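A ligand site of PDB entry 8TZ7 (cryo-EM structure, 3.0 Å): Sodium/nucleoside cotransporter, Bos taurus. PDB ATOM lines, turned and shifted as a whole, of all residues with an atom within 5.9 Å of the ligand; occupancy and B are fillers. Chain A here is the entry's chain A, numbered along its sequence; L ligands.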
ATOM      1  N   TRP A 191     -18.520  23.966  31.815  1.00  0.00           N
ATOM      2  CA  TRP A 191     -17.368  24.012  30.925  1.00  0.00           C
ATOM      3  C   TRP A 191     -16.092  23.567  31.642  1.00  0.00           C
ATOM      4  O   TRP A 191     -15.204  22.955  31.022  1.00  0.00           O
ATOM      5  CB  TRP A 191     -17.192  25.424  30.363  1.00  0.00           C
ATOM      6  CG  TRP A 191     -16.061  25.530  29.396  1.00  0.00           C
ATOM      7  CD1 TRP A 191     -15.006  26.389  29.452  1.00  0.00           C
ATOM      8  CD2 TRP A 191     -15.854  24.725  28.227  1.00  0.00           C
ATOM      9  NE1 TRP A 191     -14.158  26.186  28.396  1.00  0.00           N
ATOM     10  CE2 TRP A 191     -14.658  25.159  27.626  1.00  0.00           C
ATOM     11  CE3 TRP A 191     -16.571  23.686  27.628  1.00  0.00           C
ATOM     12  CZ2 TRP A 191     -14.161  24.595  26.447  1.00  0.00           C
ATOM     13  CZ3 TRP A 191     -16.077  23.124  26.474  1.00  0.00           C
ATOM     14  CH2 TRP A 191     -14.885  23.576  25.896  1.00  0.00           C
ATOM     15  N   ILE A 198     -13.507  17.257  26.170  1.00  0.00           N
ATOM     16  CA  ILE A 198     -13.539  17.608  24.752  1.00  0.00           C
ATOM     17  C   ILE A 198     -12.140  17.512  24.153  1.00  0.00           C
ATOM     18  O   ILE A 198     -11.951  16.948  23.059  1.00  0.00           O
ATOM     19  CB  ILE A 198     -14.152  18.996  24.560  1.00  0.00           C
ATOM     20  CG1 ILE A 198     -15.618  19.018  24.990  1.00  0.00           C
ATOM     21  CG2 ILE A 198     -14.017  19.460  23.114  1.00  0.00           C
ATOM     22  CD1 ILE A 198     -16.525  18.105  24.186  1.00  0.00           C
ATOM     23  N   TRP A 199     -11.142  18.057  24.852  1.00  0.00           N
ATOM     24  CA  TRP A 199      -9.777  18.024  24.338  1.00  0.00           C
ATOM     25  C   TRP A 199      -9.287  16.584  24.193  1.00  0.00           C
ATOM     26  O   TRP A 199      -8.655  16.225  23.192  1.00  0.00           O
ATOM     27  CB  TRP A 199      -8.857  18.832  25.254  1.00  0.00           C
ATOM     28  CG  TRP A 199      -9.252  20.288  25.347  1.00  0.00           C
ATOM     29  CD1 TRP A 199     -10.058  20.972  24.493  1.00  0.00           C
ATOM     30  CD2 TRP A 199      -8.854  21.216  26.363  1.00  0.00           C
ATOM     31  NE1 TRP A 199     -10.196  22.270  24.904  1.00  0.00           N
ATOM     32  CE2 TRP A 199      -9.461  22.449  26.051  1.00  0.00           C
ATOM     33  CE3 TRP A 199      -8.047  21.131  27.499  1.00  0.00           C
ATOM     34  CZ2 TRP A 199      -9.288  23.595  26.834  1.00  0.00           C
ATOM     35  CZ3 TRP A 199      -7.882  22.266  28.278  1.00  0.00           C
ATOM     36  CH2 TRP A 199      -8.498  23.480  27.940  1.00  0.00           C
ATOM     37  N   LEU A 202     -10.888  14.931  21.165  1.00  0.00           N
ATOM     38  CA  LEU A 202     -10.291  15.406  19.917  1.00  0.00           C
ATOM     39  C   LEU A 202      -8.931  14.768  19.681  1.00  0.00           C
ATOM     40  O   LEU A 202      -8.610  14.348  18.556  1.00  0.00           O
ATOM     41  CB  LEU A 202     -10.176  16.930  19.940  1.00  0.00           C
ATOM     42  CG  LEU A 202     -11.508  17.675  19.785  1.00  0.00           C
ATOM     43  CD1 LEU A 202     -11.403  19.105  20.267  1.00  0.00           C
ATOM     44  CD2 LEU A 202     -11.964  17.637  18.333  1.00  0.00           C
ATOM     45  N   GLY A 205      -9.384  11.144  18.597  1.00  0.00           N
ATOM     46  CA  GLY A 205      -9.810  11.062  17.211  1.00  0.00           C
ATOM     47  C   GLY A 205      -8.673  11.330  16.244  1.00  0.00           C
ATOM     48  O   GLY A 205      -8.538  10.628  15.227  1.00  0.00           O
ATOM     49  N   VAL A 206      -7.854  12.338  16.534  1.00  0.00           N
ATOM     50  CA  VAL A 206      -6.708  12.623  15.684  1.00  0.00           C
ATOM     51  C   VAL A 206      -5.795  11.416  15.594  1.00  0.00           C
ATOM     52  O   VAL A 206      -5.358  11.015  14.509  1.00  0.00           O
ATOM     53  CB  VAL A 206      -5.943  13.853  16.215  1.00  0.00           C
ATOM     54  CG1 VAL A 206      -4.608  14.026  15.494  1.00  0.00           C
ATOM     55  CG2 VAL A 206      -6.789  15.115  16.052  1.00  0.00           C
ATOM     56  N   TRP A 209      -7.498   8.468  13.482  1.00  0.00           N
ATOM     57  CA  TRP A 209      -7.544   8.778  12.056  1.00  0.00           C
ATOM     58  C   TRP A 209      -6.144   8.717  11.454  1.00  0.00           C
ATOM     59  O   TRP A 209      -5.930   8.085  10.406  1.00  0.00           O
ATOM     60  CB  TRP A 209      -8.152  10.153  11.823  1.00  0.00           C
ATOM     61  CG  TRP A 209      -7.856  10.712  10.466  1.00  0.00           C
ATOM     62  CD1 TRP A 209      -6.792  11.488  10.114  1.00  0.00           C
ATOM     63  CD2 TRP A 209      -8.629  10.527   9.279  1.00  0.00           C
ATOM     64  NE1 TRP A 209      -6.860  11.809   8.778  1.00  0.00           N
ATOM     65  CE2 TRP A 209      -7.981  11.219   8.240  1.00  0.00           C
ATOM     66  CE3 TRP A 209      -9.816   9.843   8.987  1.00  0.00           C
ATOM     67  CZ2 TRP A 209      -8.467  11.259   6.940  1.00  0.00           C
ATOM     68  CZ3 TRP A 209     -10.305   9.872   7.696  1.00  0.00           C
ATOM     69  CH2 TRP A 209      -9.632  10.581   6.685  1.00  0.00           C
ATOM     70  N   TYR A 246      -2.483  33.086  21.857  1.00  0.00           N
ATOM     71  CA  TYR A 246      -3.812  32.494  21.947  1.00  0.00           C
ATOM     72  C   TYR A 246      -3.854  31.311  20.981  1.00  0.00           C
ATOM     73  O   TYR A 246      -3.697  31.483  19.770  1.00  0.00           O
ATOM     74  CB  TYR A 246      -4.875  33.532  21.622  1.00  0.00           C
ATOM     75  CG  TYR A 246      -6.294  33.175  22.040  1.00  0.00           C
ATOM     76  CD1 TYR A 246      -6.540  32.232  23.029  1.00  0.00           C
ATOM     77  CD2 TYR A 246      -7.382  33.801  21.436  1.00  0.00           C
ATOM     78  CE1 TYR A 246      -7.829  31.919  23.405  1.00  0.00           C
ATOM     79  CE2 TYR A 246      -8.670  33.488  21.812  1.00  0.00           C
ATOM     80  CZ  TYR A 246      -8.893  32.561  22.791  1.00  0.00           C
ATOM     81  OH  TYR A 246     -10.187  32.254  23.161  1.00  0.00           O
ATOM     82  N   TRP A 247      -4.033  30.100  21.523  1.00  0.00           N
ATOM     83  CA  TRP A 247      -3.938  28.883  20.719  1.00  0.00           C
ATOM     84  C   TRP A 247      -5.231  28.513  20.018  1.00  0.00           C
ATOM     85  O   TRP A 247      -5.205  27.709  19.068  1.00  0.00           O
ATOM     86  CB  TRP A 247      -3.486  27.726  21.605  1.00  0.00           C
ATOM     87  CG  TRP A 247      -2.036  27.812  21.962  1.00  0.00           C
ATOM     88  CD1 TRP A 247      -1.511  28.188  23.167  1.00  0.00           C
ATOM     89  CD2 TRP A 247      -0.925  27.526  21.113  1.00  0.00           C
ATOM     90  NE1 TRP A 247      -0.139  28.148  23.111  1.00  0.00           N
ATOM     91  CE2 TRP A 247       0.247  27.748  21.863  1.00  0.00           C
ATOM     92  CE3 TRP A 247      -0.806  27.099  19.784  1.00  0.00           C
ATOM     93  CZ2 TRP A 247       1.517  27.556  21.322  1.00  0.00           C
ATOM     94  CZ3 TRP A 247       0.455  26.914  19.261  1.00  0.00           C
ATOM     95  CH2 TRP A 247       1.602  27.144  20.028  1.00  0.00           C
ATOM     96  N   ARG A 248      -6.364  29.064  20.460  1.00  0.00           N
ATOM     97  CA  ARG A 248      -7.635  28.748  19.810  1.00  0.00           C
ATOM     98  C   ARG A 248      -7.629  29.105  18.340  1.00  0.00           C
ATOM     99  O   ARG A 248      -8.062  28.281  17.507  1.00  0.00           O
ATOM    100  CB  ARG A 248      -8.767  29.447  20.571  1.00  0.00           C
ATOM    101  CG  ARG A 248     -10.165  29.087  20.105  1.00  0.00           C
ATOM    102  CD  ARG A 248     -11.189  30.077  20.636  1.00  0.00           C
ATOM    103  NE  ARG A 248     -12.533  29.760  20.156  1.00  0.00           N
ATOM    104  CZ  ARG A 248     -13.579  30.573  20.233  1.00  0.00           C
ATOM    105  NH1 ARG A 248     -13.472  31.775  20.782  1.00  0.00           N
ATOM    106  NH2 ARG A 248     -14.756  30.169  19.770  1.00  0.00           N
ATOM    107  N   PHE A 251      -5.398  26.360  16.435  1.00  0.00           N
ATOM    108  CA  PHE A 251      -6.008  25.041  16.371  1.00  0.00           C
ATOM    109  C   PHE A 251      -7.232  25.034  15.467  1.00  0.00           C
ATOM    110  O   PHE A 251      -7.410  24.135  14.641  1.00  0.00           O
ATOM    111  CB  PHE A 251      -6.367  24.568  17.779  1.00  0.00           C
ATOM    112  CG  PHE A 251      -5.181  24.127  18.597  1.00  0.00           C
ATOM    113  CD1 PHE A 251      -4.229  23.279  18.059  1.00  0.00           C
ATOM    114  CD2 PHE A 251      -5.021  24.576  19.898  1.00  0.00           C
ATOM    115  CE1 PHE A 251      -3.136  22.879  18.805  1.00  0.00           C
ATOM    116  CE2 PHE A 251      -3.929  24.176  20.644  1.00  0.00           C
ATOM    117  CZ  PHE A 251      -2.990  23.328  20.103  1.00  0.00           C
ATOM    118  N   TRP A 252      -8.085  26.055  15.586  1.00  0.00           N
ATOM    119  CA  TRP A 252      -9.281  26.120  14.745  1.00  0.00           C
ATOM    120  C   TRP A 252      -8.923  26.318  13.286  1.00  0.00           C
ATOM    121  O   TRP A 252      -9.581  25.761  12.401  1.00  0.00           O
ATOM    122  CB  TRP A 252     -10.202  27.237  15.241  1.00  0.00           C
ATOM    123  CG  TRP A 252     -11.243  26.737  16.187  1.00  0.00           C
ATOM    124  CD1 TRP A 252     -11.300  26.948  17.530  1.00  0.00           C
ATOM    125  CD2 TRP A 252     -12.371  25.920  15.855  1.00  0.00           C
ATOM    126  NE1 TRP A 252     -12.404  26.316  18.058  1.00  0.00           N
ATOM    127  CE2 TRP A 252     -13.071  25.678  17.043  1.00  0.00           C
ATOM    128  CE3 TRP A 252     -12.847  25.364  14.660  1.00  0.00           C
ATOM    129  CZ2 TRP A 252     -14.240  24.916  17.086  1.00  0.00           C
ATOM    130  CZ3 TRP A 252     -13.994  24.606  14.703  1.00  0.00           C
ATOM    131  CH2 TRP A 252     -14.680  24.387  15.900  1.00  0.00           C
ATOM    132  N   GLY A 255      -7.844  22.963  11.986  1.00  0.00           N
ATOM    133  CA  GLY A 255      -8.989  22.087  11.866  1.00  0.00           C
ATOM    134  C   GLY A 255      -9.871  22.422  10.674  1.00  0.00           C
ATOM    135  O   GLY A 255     -10.334  21.523   9.960  1.00  0.00           O
ATOM    136  N   LEU A 256     -10.132  23.702  10.451  1.00  0.00           N
ATOM    137  CA  LEU A 256     -10.949  24.106   9.316  1.00  0.00           C
ATOM    138  C   LEU A 256     -10.255  23.769   7.997  1.00  0.00           C
ATOM    139  O   LEU A 256     -10.905  23.313   7.045  1.00  0.00           O
ATOM    140  CB  LEU A 256     -11.283  25.594   9.393  1.00  0.00           C
ATOM    141  CG  LEU A 256     -12.149  26.040  10.561  1.00  0.00           C
ATOM    142  CD1 LEU A 256     -12.348  27.546  10.527  1.00  0.00           C
ATOM    143  CD2 LEU A 256     -13.501  25.336  10.558  1.00  0.00           C
ATOM    144  N   PHE A 258      -8.255  21.270   7.536  1.00  0.00           N
ATOM    145  CA  PHE A 258      -8.366  19.833   7.381  1.00  0.00           C
ATOM    146  C   PHE A 258      -9.756  19.437   6.906  1.00  0.00           C
ATOM    147  O   PHE A 258      -9.894  18.580   6.026  1.00  0.00           O
ATOM    148  CB  PHE A 258      -8.027  19.134   8.695  1.00  0.00           C
ATOM    149  CG  PHE A 258      -8.189  17.653   8.659  1.00  0.00           C
ATOM    150  CD1 PHE A 258      -7.194  16.844   8.133  1.00  0.00           C
ATOM    151  CD2 PHE A 258      -9.334  17.055   9.140  1.00  0.00           C
ATOM    152  CE1 PHE A 258      -7.345  15.477   8.096  1.00  0.00           C
ATOM    153  CE2 PHE A 258      -9.492  15.683   9.106  1.00  0.00           C
ATOM    154  CZ  PHE A 258      -8.497  14.891   8.580  1.00  0.00           C
ATOM    155  N   LEU A 259     -10.786  20.042   7.473  1.00  0.00           N
ATOM    156  CA  LEU A 259     -12.152  19.695   7.079  1.00  0.00           C
ATOM    157  C   LEU A 259     -12.429  20.072   5.630  1.00  0.00           C
ATOM    158  O   LEU A 259     -13.002  19.275   4.872  1.00  0.00           O
ATOM    159  CB  LEU A 259     -13.159  20.351   8.021  1.00  0.00           C
ATOM    160  CG  LEU A 259     -13.164  19.818   9.451  1.00  0.00           C
ATOM    161  CD1 LEU A 259     -14.103  20.636  10.325  1.00  0.00           C
ATOM    162  CD2 LEU A 259     -13.569  18.351   9.496  1.00  0.00           C
ATOM    163  N   LEU A 262     -10.500  17.694   3.388  1.00  0.00           N
ATOM    164  CA  LEU A 262     -11.091  16.362   3.416  1.00  0.00           C
ATOM    165  C   LEU A 262     -12.329  16.299   2.542  1.00  0.00           C
ATOM    166  O   LEU A 262     -12.463  15.425   1.676  1.00  0.00           O
ATOM    167  CB  LEU A 262     -11.417  15.976   4.862  1.00  0.00           C
ATOM    168  CG  LEU A 262     -11.585  14.495   5.197  1.00  0.00           C
ATOM    169  CD1 LEU A 262     -10.280  13.748   5.053  1.00  0.00           C
ATOM    170  CD2 LEU A 262     -12.134  14.326   6.606  1.00  0.00           C
HETATM  171  C1  LIG L   1     -12.623  27.264  24.019  1.00  0.00           C
HETATM  172  P1  LIG L   1     -12.292  29.820  24.548  1.00  0.00           P
HETATM  173  C2  LIG L   1     -12.058  26.287  22.987  1.00  0.00           C
HETATM  174  C3  LIG L   1     -13.086  25.993  21.929  1.00  0.00           C
HETATM  175  C4  LIG L   1     -11.757  20.000  13.216  1.00  0.00           C
HETATM  176  O1  LIG L   1     -12.615  28.569  23.492  1.00  0.00           O
HETATM  177  C5  LIG L   1     -11.898  18.639  13.922  1.00  0.00           C
HETATM  178  O2  LIG L   1     -10.840  29.775  24.945  1.00  0.00           O
HETATM  179  C6  LIG L   1     -11.239  17.517  13.072  1.00  0.00           C
HETATM  180  O3  LIG L   1     -12.591  31.144  23.885  1.00  0.00           O
HETATM  181  C7  LIG L   1     -10.235  16.720  13.916  1.00  0.00           C
HETATM  182  O4  LIG L   1     -13.238  29.653  25.885  1.00  0.00           O
HETATM  183  C8  LIG L   1      -9.659  15.525  13.150  1.00  0.00           C
HETATM  184  C9  LIG L   1     -10.256  14.209  13.640  1.00  0.00           C
HETATM  185  C10 LIG L   1      -9.899  13.051  12.736  1.00  0.00           C
HETATM  186  C11 LIG L   1     -10.856  12.938  11.556  1.00  0.00           C
HETATM  187  C12 LIG L   1     -11.844  11.809  11.724  1.00  0.00           C
HETATM  188  C13 LIG L   1     -14.019  23.826  21.981  1.00  0.00           C
HETATM  189  O5  LIG L   1     -14.045  25.147  22.493  1.00  0.00           O
HETATM  190  C14 LIG L   1     -14.992  23.416  20.869  1.00  0.00           C
HETATM  191  O6  LIG L   1     -13.245  23.037  22.413  1.00  0.00           O
HETATM  192  C15 LIG L   1     -14.477  22.220  20.043  1.00  0.00           C
HETATM  193  C16 LIG L   1     -15.521  21.715  19.036  1.00  0.00           C
HETATM  194  C17 LIG L   1     -14.952  20.617  18.127  1.00  0.00           C
HETATM  195  C18 LIG L   1     -15.704  20.505  16.795  1.00  0.00           C
HETATM  196  C19 LIG L   1     -15.188  19.336  15.923  1.00  0.00           C
HETATM  197  C20 LIG L   1      -9.743  26.000  22.490  1.00  0.00           C
HETATM  198  O7  LIG L   1     -10.901  26.832  22.381  1.00  0.00           O
HETATM  199  C21 LIG L   1      -9.761  24.587  21.839  1.00  0.00           C
HETATM  200  O8  LIG L   1      -8.792  26.369  23.091  1.00  0.00           O
HETATM  201  C22 LIG L   1      -9.673  24.642  20.288  1.00  0.00           C
HETATM  202  C23 LIG L   1     -10.485  23.491  19.675  1.00  0.00           C
HETATM  203  C24 LIG L   1     -10.142  23.215  18.206  1.00  0.00           C
HETATM  204  C25 LIG L   1     -11.203  22.317  17.549  1.00  0.00           C
HETATM  205  C26 LIG L   1     -10.923  22.031  16.065  1.00  0.00           C
HETATM  206  C27 LIG L   1     -12.106  21.287  15.396  1.00  0.00           C
HETATM  207  C28 LIG L   1     -11.848  21.180  13.870  1.00  0.00           C
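An oxygen (O3) of the ligand is in hydrogen-bond range of the side-chain hydroxyl (OH) of Tyr 246.
NH1 of Arg 248 lies within salt-bridge range of O3 of the ligand, at 3.3 Å.
Residues that only touch the ligand: Trp 191 (3.8 Å), Ile 198 (3.7 Å), Trp 199 (3.9 Å), Gly 205 (3.7 Å), Trp 209 (3.5 Å), Trp 252 (3.8 Å), Gly 255 (3.6 Å), Phe 258 (3.9 Å) and Leu 259 (3.8 Å).
Hydrophobic or aromatic side chains that line the ligand: Trp 191, Ile 198, Trp 209, Trp 252, Phe 258 and Leu 259.
11 residues have an atom within 4 Å of the ligand: Trp 191, Ile 198, Trp 199, Gly 205, Trp 209, Tyr 246, Arg 248, Trp 252, Gly 255, Phe 258 and Leu 259.
The nearest printed residue that does not touch the ligand is Phe 251 (4.03 Å).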
